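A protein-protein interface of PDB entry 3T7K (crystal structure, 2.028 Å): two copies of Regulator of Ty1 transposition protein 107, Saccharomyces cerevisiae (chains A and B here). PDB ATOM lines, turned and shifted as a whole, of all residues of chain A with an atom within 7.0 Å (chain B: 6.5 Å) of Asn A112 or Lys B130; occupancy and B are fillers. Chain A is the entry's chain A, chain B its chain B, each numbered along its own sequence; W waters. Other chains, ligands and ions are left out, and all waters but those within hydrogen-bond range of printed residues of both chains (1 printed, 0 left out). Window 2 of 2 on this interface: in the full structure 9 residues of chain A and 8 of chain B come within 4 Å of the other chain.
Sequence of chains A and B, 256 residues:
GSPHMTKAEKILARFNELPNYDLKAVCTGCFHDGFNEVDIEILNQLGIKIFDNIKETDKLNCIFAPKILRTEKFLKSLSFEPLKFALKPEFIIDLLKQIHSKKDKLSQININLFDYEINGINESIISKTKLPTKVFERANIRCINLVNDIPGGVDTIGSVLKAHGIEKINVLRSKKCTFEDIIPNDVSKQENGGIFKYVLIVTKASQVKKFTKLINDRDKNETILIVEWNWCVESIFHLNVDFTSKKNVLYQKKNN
The side-chain amide oxygen (OD1) of Asn A112 is in hydrogen-bond range of the backbone NH (N) of Phe A114, at 2.9 Å.
The side-chain hydroxyl of Tyr A21 sits at hydrogen-bond distance from the backbone carbonyl oxygen of Ile A111 (2.7 Å).
N of Asp A115 sits at hydrogen-bond distance from OD1 of Asn A112, 2.9 Å away.
Tyr A21 touches Pro B132.
Asn A110 touches Leu B131 (CB to CD2, 3.7 Å).
Ile A111 touches Pro B132.
Lys B130 touches Asn A112.
CE1 of Phe A114 touches O of Glu B81 (3.5 Å).
Lys B130 touches Phe A114 (O to CE2, 3.4 Å).
Of chain B, only Lys B130 (3.1 Å) comes within 4 Å of Asn A112.
Of chain A, only Asn A112 (3.1 Å) and Phe A114 (3.4 Å) come within 4 Å of Lys B130.
Of the printed residues of chain A, Pro B132 touches Tyr A21 and Ile A111.
Printed residues of chain B within 4 Å of Phe A114: Glu B81 (3.5 Å) and Lys B130 (3.4 Å).
Asp A115 touches none of the printed residues of chain B.
The nearest residue of chain A that does not touch Lys B130 is Asp A115 (4.4 Å).
The nearest printed residue of chain B that does not touch Asn A110 is Pro B132 (4.2 Å).
Of the 13 printed residues of chain B, 4 touch a printed residue of chain A.
Of the 11 printed residues of chain A, 5 touch a printed residue of chain B.
Printed residues of chain A that touch a printed residue of chain B: Tyr A21, Asn A110, Ile A111, Asn A112 and Phe A114.
Among the printed residues, no Asp or Glu carboxylate lies within 4 Å of a Lys or Arg side-chain nitrogen of the other chain.
No position is printed for both chains.
Water W1 bridges O of Lys B130 (2.8 Å) and N of Leu A113 (2.9 Å).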
ATOM      1  N   TYR A  21     -21.722 -17.034  27.067  1.00  0.00           N
ATOM      2  CA  TYR A  21     -21.155 -15.844  27.730  1.00  0.00           C
ATOM      3  C   TYR A  21     -19.638 -15.773  27.636  1.00  0.00           C
ATOM      4  O   TYR A  21     -19.045 -14.719  27.908  1.00  0.00           O
ATOM      5  CB  TYR A  21     -21.607 -15.765  29.195  1.00  0.00           C
ATOM      6  CG  TYR A  21     -23.055 -15.421  29.370  1.00  0.00           C
ATOM      7  CD1 TYR A  21     -23.497 -14.118  29.255  1.00  0.00           C
ATOM      8  CD2 TYR A  21     -23.989 -16.409  29.637  1.00  0.00           C
ATOM      9  CE1 TYR A  21     -24.842 -13.804  29.402  1.00  0.00           C
ATOM     10  CE2 TYR A  21     -25.319 -16.109  29.791  1.00  0.00           C
ATOM     11  CZ  TYR A  21     -25.746 -14.817  29.664  1.00  0.00           C
ATOM     12  OH  TYR A  21     -27.082 -14.538  29.830  1.00  0.00           O
ATOM     13  N   LEU A  87     -17.424  -8.561  37.221  1.00  0.00           N
ATOM     14  CA  LEU A  87     -18.864  -8.576  37.425  1.00  0.00           C
ATOM     15  C   LEU A  87     -19.258  -8.856  38.865  1.00  0.00           C
ATOM     16  O   LEU A  87     -18.580  -9.603  39.564  1.00  0.00           O
ATOM     17  CB  LEU A  87     -19.489  -9.667  36.547  1.00  0.00           C
ATOM     18  CG  LEU A  87     -19.317  -9.522  35.038  1.00  0.00           C
ATOM     19  CD1 LEU A  87     -19.943 -10.718  34.340  1.00  0.00           C
ATOM     20  CD2 LEU A  87     -19.951  -8.234  34.559  1.00  0.00           C
ATOM     21  N   PHE A  91     -24.901 -11.324  38.772  1.00  0.00           N
ATOM     22  CA  PHE A  91     -24.992 -11.846  37.420  1.00  0.00           C
ATOM     23  C   PHE A  91     -25.285 -13.348  37.425  1.00  0.00           C
ATOM     24  O   PHE A  91     -26.221 -13.805  36.764  1.00  0.00           O
ATOM     25  CB  PHE A  91     -23.719 -11.576  36.623  1.00  0.00           C
ATOM     26  CG  PHE A  91     -23.649 -12.350  35.346  1.00  0.00           C
ATOM     27  CD1 PHE A  91     -24.327 -11.908  34.219  1.00  0.00           C
ATOM     28  CD2 PHE A  91     -22.933 -13.530  35.276  1.00  0.00           C
ATOM     29  CE1 PHE A  91     -24.286 -12.630  33.038  1.00  0.00           C
ATOM     30  CE2 PHE A  91     -22.886 -14.262  34.101  1.00  0.00           C
ATOM     31  CZ  PHE A  91     -23.565 -13.810  32.978  1.00  0.00           C
ATOM     32  N   ILE A 109     -33.425 -16.514  27.673  1.00  0.00           N
ATOM     33  CA  ILE A 109     -32.420 -16.010  28.613  1.00  0.00           C
ATOM     34  C   ILE A 109     -31.937 -14.642  28.157  1.00  0.00           C
ATOM     35  O   ILE A 109     -31.451 -14.491  27.049  1.00  0.00           O
ATOM     36  CB  ILE A 109     -31.225 -16.969  28.688  1.00  0.00           C
ATOM     37  CG1 ILE A 109     -31.693 -18.346  29.158  1.00  0.00           C
ATOM     38  CG2 ILE A 109     -30.146 -16.419  29.607  1.00  0.00           C
ATOM     39  CD1 ILE A 109     -30.647 -19.435  29.021  1.00  0.00           C
ATOM     40  N   ASN A 110     -32.071 -13.639  29.012  1.00  0.00           N
ATOM     41  CA  ASN A 110     -31.766 -12.283  28.598  1.00  0.00           C
ATOM     42  C   ASN A 110     -30.853 -11.547  29.570  1.00  0.00           C
ATOM     43  O   ASN A 110     -30.681 -10.340  29.474  1.00  0.00           O
ATOM     44  CB  ASN A 110     -33.061 -11.507  28.420  1.00  0.00           C
ATOM     45  CG  ASN A 110     -33.972 -11.648  29.607  1.00  0.00           C
ATOM     46  OD1 ASN A 110     -33.552 -11.444  30.744  1.00  0.00           O
ATOM     47  ND2 ASN A 110     -35.219 -12.046  29.360  1.00  0.00           N
ATOM     48  N   ILE A 111     -30.273 -12.271  30.514  1.00  0.00           N
ATOM     49  CA  ILE A 111     -29.318 -11.657  31.421  1.00  0.00           C
ATOM     50  C   ILE A 111     -28.096 -11.141  30.664  1.00  0.00           C
ATOM     51  O   ILE A 111     -27.435 -11.898  29.941  1.00  0.00           O
ATOM     52  CB  ILE A 111     -28.883 -12.635  32.504  1.00  0.00           C
ATOM     53  CG1 ILE A 111     -30.120 -13.255  33.161  1.00  0.00           C
ATOM     54  CG2 ILE A 111     -28.004 -11.924  33.533  1.00  0.00           C
ATOM     55  CD1 ILE A 111     -31.066 -12.235  33.754  1.00  0.00           C
ATOM     56  N   ASN A 112     -27.796  -9.854  30.825  1.00  0.00           N
ATOM     57  CA  ASN A 112     -26.704  -9.230  30.078  1.00  0.00           C
ATOM     58  C   ASN A 112     -25.441  -8.946  30.896  1.00  0.00           C
ATOM     59  O   ASN A 112     -25.472  -8.882  32.121  1.00  0.00           O
ATOM     60  CB  ASN A 112     -27.173  -7.958  29.368  1.00  0.00           C
ATOM     61  CG  ASN A 112     -27.506  -6.835  30.324  1.00  0.00           C
ATOM     62  OD1 ASN A 112     -26.609  -6.172  30.866  1.00  0.00           O
ATOM     63  ND2 ASN A 112     -28.800  -6.595  30.521  1.00  0.00           N
ATOM     64  N   LEU A 113     -24.333  -8.768  30.191  1.00  0.00           N
ATOM     65  CA  LEU A 113     -23.028  -8.606  30.816  1.00  0.00           C
ATOM     66  C   LEU A 113     -22.702  -7.145  31.111  1.00  0.00           C
ATOM     67  O   LEU A 113     -21.542  -6.813  31.355  1.00  0.00           O
ATOM     68  CB  LEU A 113     -21.945  -9.149  29.884  1.00  0.00           C
ATOM     69  CG  LEU A 113     -21.916 -10.643  29.597  1.00  0.00           C
ATOM     70  CD1 LEU A 113     -21.181 -10.894  28.301  1.00  0.00           C
ATOM     71  CD2 LEU A 113     -21.244 -11.372  30.750  1.00  0.00           C
ATOM     72  N   PHE A 114     -23.700  -6.270  31.076  1.00  0.00           N
ATOM     73  CA  PHE A 114     -23.432  -4.844  31.229  1.00  0.00           C
ATOM     74  C   PHE A 114     -24.090  -4.267  32.476  1.00  0.00           C
ATOM     75  O   PHE A 114     -23.690  -3.214  32.970  1.00  0.00           O
ATOM     76  CB  PHE A 114     -23.881  -4.065  29.988  1.00  0.00           C
ATOM     77  CG  PHE A 114     -23.417  -4.666  28.700  1.00  0.00           C
ATOM     78  CD1 PHE A 114     -22.087  -4.568  28.315  1.00  0.00           C
ATOM     79  CD2 PHE A 114     -24.304  -5.346  27.878  1.00  0.00           C
ATOM     80  CE1 PHE A 114     -21.652  -5.136  27.128  1.00  0.00           C
ATOM     81  CE2 PHE A 114     -23.881  -5.912  26.683  1.00  0.00           C
ATOM     82  CZ  PHE A 114     -22.558  -5.814  26.306  1.00  0.00           C
ATOM     83  N   ASP A 115     -25.101  -4.955  32.985  1.00  0.00           N
ATOM     84  CA  ASP A 115     -25.845  -4.436  34.119  1.00  0.00           C
ATOM     85  C   ASP A 115     -25.289  -4.884  35.461  1.00  0.00           C
ATOM     86  O   ASP A 115     -25.977  -4.787  36.471  1.00  0.00           O
ATOM     87  CB  ASP A 115     -27.313  -4.833  34.007  1.00  0.00           C
ATOM     88  CG  ASP A 115     -28.000  -4.129  32.878  1.00  0.00           C
ATOM     89  OD1 ASP A 115     -29.136  -4.512  32.509  1.00  0.00           O
ATOM     90  OD2 ASP A 115     -27.369  -3.192  32.351  1.00  0.00           O
ATOM     91  N   TYR A 116     -24.052  -5.368  35.475  1.00  0.00           N
ATOM     92  CA  TYR A 116     -23.484  -5.914  36.700  1.00  0.00           C
ATOM     93  C   TYR A 116     -22.045  -5.501  36.949  1.00  0.00           C
ATOM     94  O   TYR A 116     -21.254  -6.289  37.462  1.00  0.00           O
ATOM     95  CB  TYR A 116     -23.585  -7.431  36.705  1.00  0.00           C
ATOM     96  CG  TYR A 116     -24.990  -7.926  36.501  1.00  0.00           C
ATOM     97  CD1 TYR A 116     -25.878  -8.032  37.566  1.00  0.00           C
ATOM     98  CD2 TYR A 116     -25.432  -8.284  35.239  1.00  0.00           C
ATOM     99  CE1 TYR A 116     -27.171  -8.492  37.374  1.00  0.00           C
ATOM    100  CE2 TYR A 116     -26.714  -8.746  35.033  1.00  0.00           C
ATOM    101  CZ  TYR A 116     -27.580  -8.848  36.094  1.00  0.00           C
ATOM    102  OH  TYR A 116     -28.859  -9.306  35.861  1.00  0.00           O
ATOM    103  N   PHE B  80     -23.823  -3.301  17.876  1.00  0.00           N
ATOM    104  CA  PHE B  80     -22.868  -2.763  18.830  1.00  0.00           C
ATOM    105  C   PHE B  80     -23.118  -3.415  20.196  1.00  0.00           C
ATOM    106  O   PHE B  80     -24.209  -3.941  20.458  1.00  0.00           O
ATOM    107  CB  PHE B  80     -22.969  -1.239  18.904  1.00  0.00           C
ATOM    108  CG  PHE B  80     -22.415  -0.533  17.699  1.00  0.00           C
ATOM    109  CD1 PHE B  80     -21.824  -1.244  16.671  1.00  0.00           C
ATOM    110  CD2 PHE B  80     -22.472   0.843  17.603  1.00  0.00           C
ATOM    111  CE1 PHE B  80     -21.313  -0.589  15.554  1.00  0.00           C
ATOM    112  CE2 PHE B  80     -21.968   1.508  16.503  1.00  0.00           C
ATOM    113  CZ  PHE B  80     -21.384   0.785  15.470  1.00  0.00           C
ATOM    114  N   GLU B  81     -22.116  -3.375  21.069  1.00  0.00           N
ATOM    115  CA  GLU B  81     -22.152  -4.132  22.315  1.00  0.00           C
ATOM    116  C   GLU B  81     -21.883  -3.290  23.574  1.00  0.00           C
ATOM    117  O   GLU B  81     -20.820  -3.401  24.194  1.00  0.00           O
ATOM    118  CB  GLU B  81     -21.146  -5.274  22.218  1.00  0.00           C
ATOM    119  CG  GLU B  81     -21.459  -6.244  21.062  1.00  0.00           C
ATOM    120  CD  GLU B  81     -20.349  -7.258  20.827  1.00  0.00           C
ATOM    121  OE1 GLU B  81     -19.421  -7.336  21.667  1.00  0.00           O
ATOM    122  OE2 GLU B  81     -20.399  -7.969  19.800  1.00  0.00           O
ATOM    123  N   PRO B  82     -22.851  -2.453  23.967  1.00  0.00           N
ATOM    124  CA  PRO B  82     -24.126  -2.287  23.275  1.00  0.00           C
ATOM    125  C   PRO B  82     -24.144  -1.027  22.436  1.00  0.00           C
ATOM    126  O   PRO B  82     -23.208  -0.221  22.499  1.00  0.00           O
ATOM    127  CB  PRO B  82     -25.102  -2.115  24.432  1.00  0.00           C
ATOM    128  CG  PRO B  82     -24.282  -1.297  25.440  1.00  0.00           C
ATOM    129  CD  PRO B  82     -22.840  -1.755  25.270  1.00  0.00           C
ATOM    130  N   LEU B  83     -25.219  -0.845  21.674  1.00  0.00           N
ATOM    131  CA  LEU B  83     -25.492   0.447  21.072  1.00  0.00           C
ATOM    132  C   LEU B  83     -26.129   1.270  22.164  1.00  0.00           C
ATOM    133  O   LEU B  83     -27.064   0.815  22.804  1.00  0.00           O
ATOM    134  CB  LEU B  83     -26.463   0.331  19.901  1.00  0.00           C
ATOM    135  CG  LEU B  83     -26.908   1.662  19.287  1.00  0.00           C
ATOM    136  CD1 LEU B  83     -25.752   2.369  18.569  1.00  0.00           C
ATOM    137  CD2 LEU B  83     -28.070   1.447  18.333  1.00  0.00           C
ATOM    138  N   ILE B 125     -35.670  -1.198  21.219  1.00  0.00           N
ATOM    139  CA  ILE B 125     -34.782  -1.792  20.235  1.00  0.00           C
ATOM    140  C   ILE B 125     -33.316  -1.585  20.621  1.00  0.00           C
ATOM    141  O   ILE B 125     -32.501  -2.510  20.531  1.00  0.00           O
ATOM    142  CB  ILE B 125     -35.077  -1.273  18.803  1.00  0.00           C
ATOM    143  CG1 ILE B 125     -34.474  -2.212  17.771  1.00  0.00           C
ATOM    144  CG2 ILE B 125     -34.556   0.138  18.609  1.00  0.00           C
ATOM    145  CD1 ILE B 125     -35.076  -3.604  17.815  1.00  0.00           C
ATOM    146  N   ILE B 126     -32.982  -0.380  21.069  1.00  0.00           N
ATOM    147  CA  ILE B 126     -31.630  -0.104  21.518  1.00  0.00           C
ATOM    148  C   ILE B 126     -31.246  -1.116  22.589  1.00  0.00           C
ATOM    149  O   ILE B 126     -30.139  -1.643  22.591  1.00  0.00           O
ATOM    150  CB  ILE B 126     -31.485   1.340  22.082  1.00  0.00           C
ATOM    151  CG1 ILE B 126     -31.263   2.346  20.950  1.00  0.00           C
ATOM    152  CG2 ILE B 126     -30.329   1.423  23.069  1.00  0.00           C
ATOM    153  CD1 ILE B 126     -31.184   3.783  21.416  1.00  0.00           C
ATOM    154  N   SER B 127     -32.173  -1.416  23.484  1.00  0.00           N
ATOM    155  CA  SER B 127     -31.845  -2.247  24.629  1.00  0.00           C
ATOM    156  C   SER B 127     -31.534  -3.692  24.257  1.00  0.00           C
ATOM    157  O   SER B 127     -30.755  -4.357  24.950  1.00  0.00           O
ATOM    158  CB  SER B 127     -32.938  -2.159  25.689  1.00  0.00           C
ATOM    159  OG  SER B 127     -34.209  -2.393  25.112  1.00  0.00           O
ATOM    160  N   LYS B 128     -32.110  -4.164  23.151  1.00  0.00           N
ATOM    161  CA  LYS B 128     -31.819  -5.504  22.651  1.00  0.00           C
ATOM    162  C   LYS B 128     -30.354  -5.710  22.268  1.00  0.00           C
ATOM    163  O   LYS B 128     -29.887  -6.849  22.189  1.00  0.00           O
ATOM    164  CB  LYS B 128     -32.705  -5.828  21.447  1.00  0.00           C
ATOM    165  CG  LYS B 128     -34.184  -5.918  21.772  1.00  0.00           C
ATOM    166  CD  LYS B 128     -34.998  -5.696  20.501  1.00  0.00           C
ATOM    167  CE  LYS B 128     -35.940  -6.852  20.208  1.00  0.00           C
ATOM    168  NZ  LYS B 128     -37.109  -6.848  21.129  1.00  0.00           N
ATOM    169  N   THR B 129     -29.625  -4.629  22.008  1.00  0.00           N
ATOM    170  CA  THR B 129     -28.194  -4.760  21.729  1.00  0.00           C
ATOM    171  C   THR B 129     -27.360  -5.172  22.956  1.00  0.00           C
ATOM    172  O   THR B 129     -26.183  -5.521  22.828  1.00  0.00           O
ATOM    173  CB  THR B 129     -27.593  -3.491  21.089  1.00  0.00           C
ATOM    174  OG1 THR B 129     -27.652  -2.386  22.013  1.00  0.00           O
ATOM    175  CG2 THR B 129     -28.354  -3.139  19.835  1.00  0.00           C
ATOM    176  N   LYS B 130     -27.977  -5.152  24.130  1.00  0.00           N
ATOM    177  CA  LYS B 130     -27.316  -5.605  25.355  1.00  0.00           C
ATOM    178  C   LYS B 130     -27.484  -7.114  25.520  1.00  0.00           C
ATOM    179  O   LYS B 130     -26.740  -7.760  26.259  1.00  0.00           O
ATOM    180  CB  LYS B 130     -27.877  -4.867  26.586  1.00  0.00           C
ATOM    181  CG  LYS B 130     -27.574  -3.383  26.603  1.00  0.00           C
ATOM    182  CD  LYS B 130     -28.055  -2.697  27.898  1.00  0.00           C
ATOM    183  CE  LYS B 130     -29.562  -2.467  27.854  1.00  0.00           C
ATOM    184  NZ  LYS B 130     -30.138  -1.939  29.136  1.00  0.00           N
ATOM    185  N   LEU B 131     -28.461  -7.688  24.824  1.00  0.00           N
ATOM    186  CA  LEU B 131     -28.660  -9.126  24.904  1.00  0.00           C
ATOM    187  C   LEU B 131     -27.343  -9.828  24.637  1.00  0.00           C
ATOM    188  O   LEU B 131     -26.520  -9.349  23.856  1.00  0.00           O
ATOM    189  CB  LEU B 131     -29.724  -9.585  23.925  1.00  0.00           C
ATOM    190  CG  LEU B 131     -31.120  -9.078  24.278  1.00  0.00           C
ATOM    191  CD1 LEU B 131     -32.094  -9.349  23.126  1.00  0.00           C
ATOM    192  CD2 LEU B 131     -31.603  -9.723  25.575  1.00  0.00           C
ATOM    193  N   PRO B 132     -27.127 -10.953  25.313  1.00  0.00           N
ATOM    194  CA  PRO B 132     -25.895 -11.739  25.216  1.00  0.00           C
ATOM    195  C   PRO B 132     -25.838 -12.569  23.929  1.00  0.00           C
ATOM    196  O   PRO B 132     -24.888 -13.331  23.741  1.00  0.00           O
ATOM    197  CB  PRO B 132     -25.987 -12.662  26.432  1.00  0.00           C
ATOM    198  CG  PRO B 132     -27.439 -12.803  26.660  1.00  0.00           C
ATOM    199  CD  PRO B 132     -28.026 -11.470  26.356  1.00  0.00           C
ATOM    200  N   THR B 133     -26.833 -12.404  23.058  1.00  0.00           N
ATOM    201  CA  THR B 133     -26.860 -13.108  21.784  1.00  0.00           C
ATOM    202  C   THR B 133     -27.056 -12.118  20.647  1.00  0.00           C
ATOM    203  O   THR B 133     -27.483 -10.979  20.874  1.00  0.00           O
ATOM    204  CB  THR B 133     -28.009 -14.135  21.737  1.00  0.00           C
ATOM    205  OG1 THR B 133     -29.256 -13.464  21.973  1.00  0.00           O
ATOM    206  CG2 THR B 133     -27.812 -15.191  22.801  1.00  0.00           C
HETATM  207  O   HOH W   1     -24.721  -9.384  27.371  1.00  0.00           O
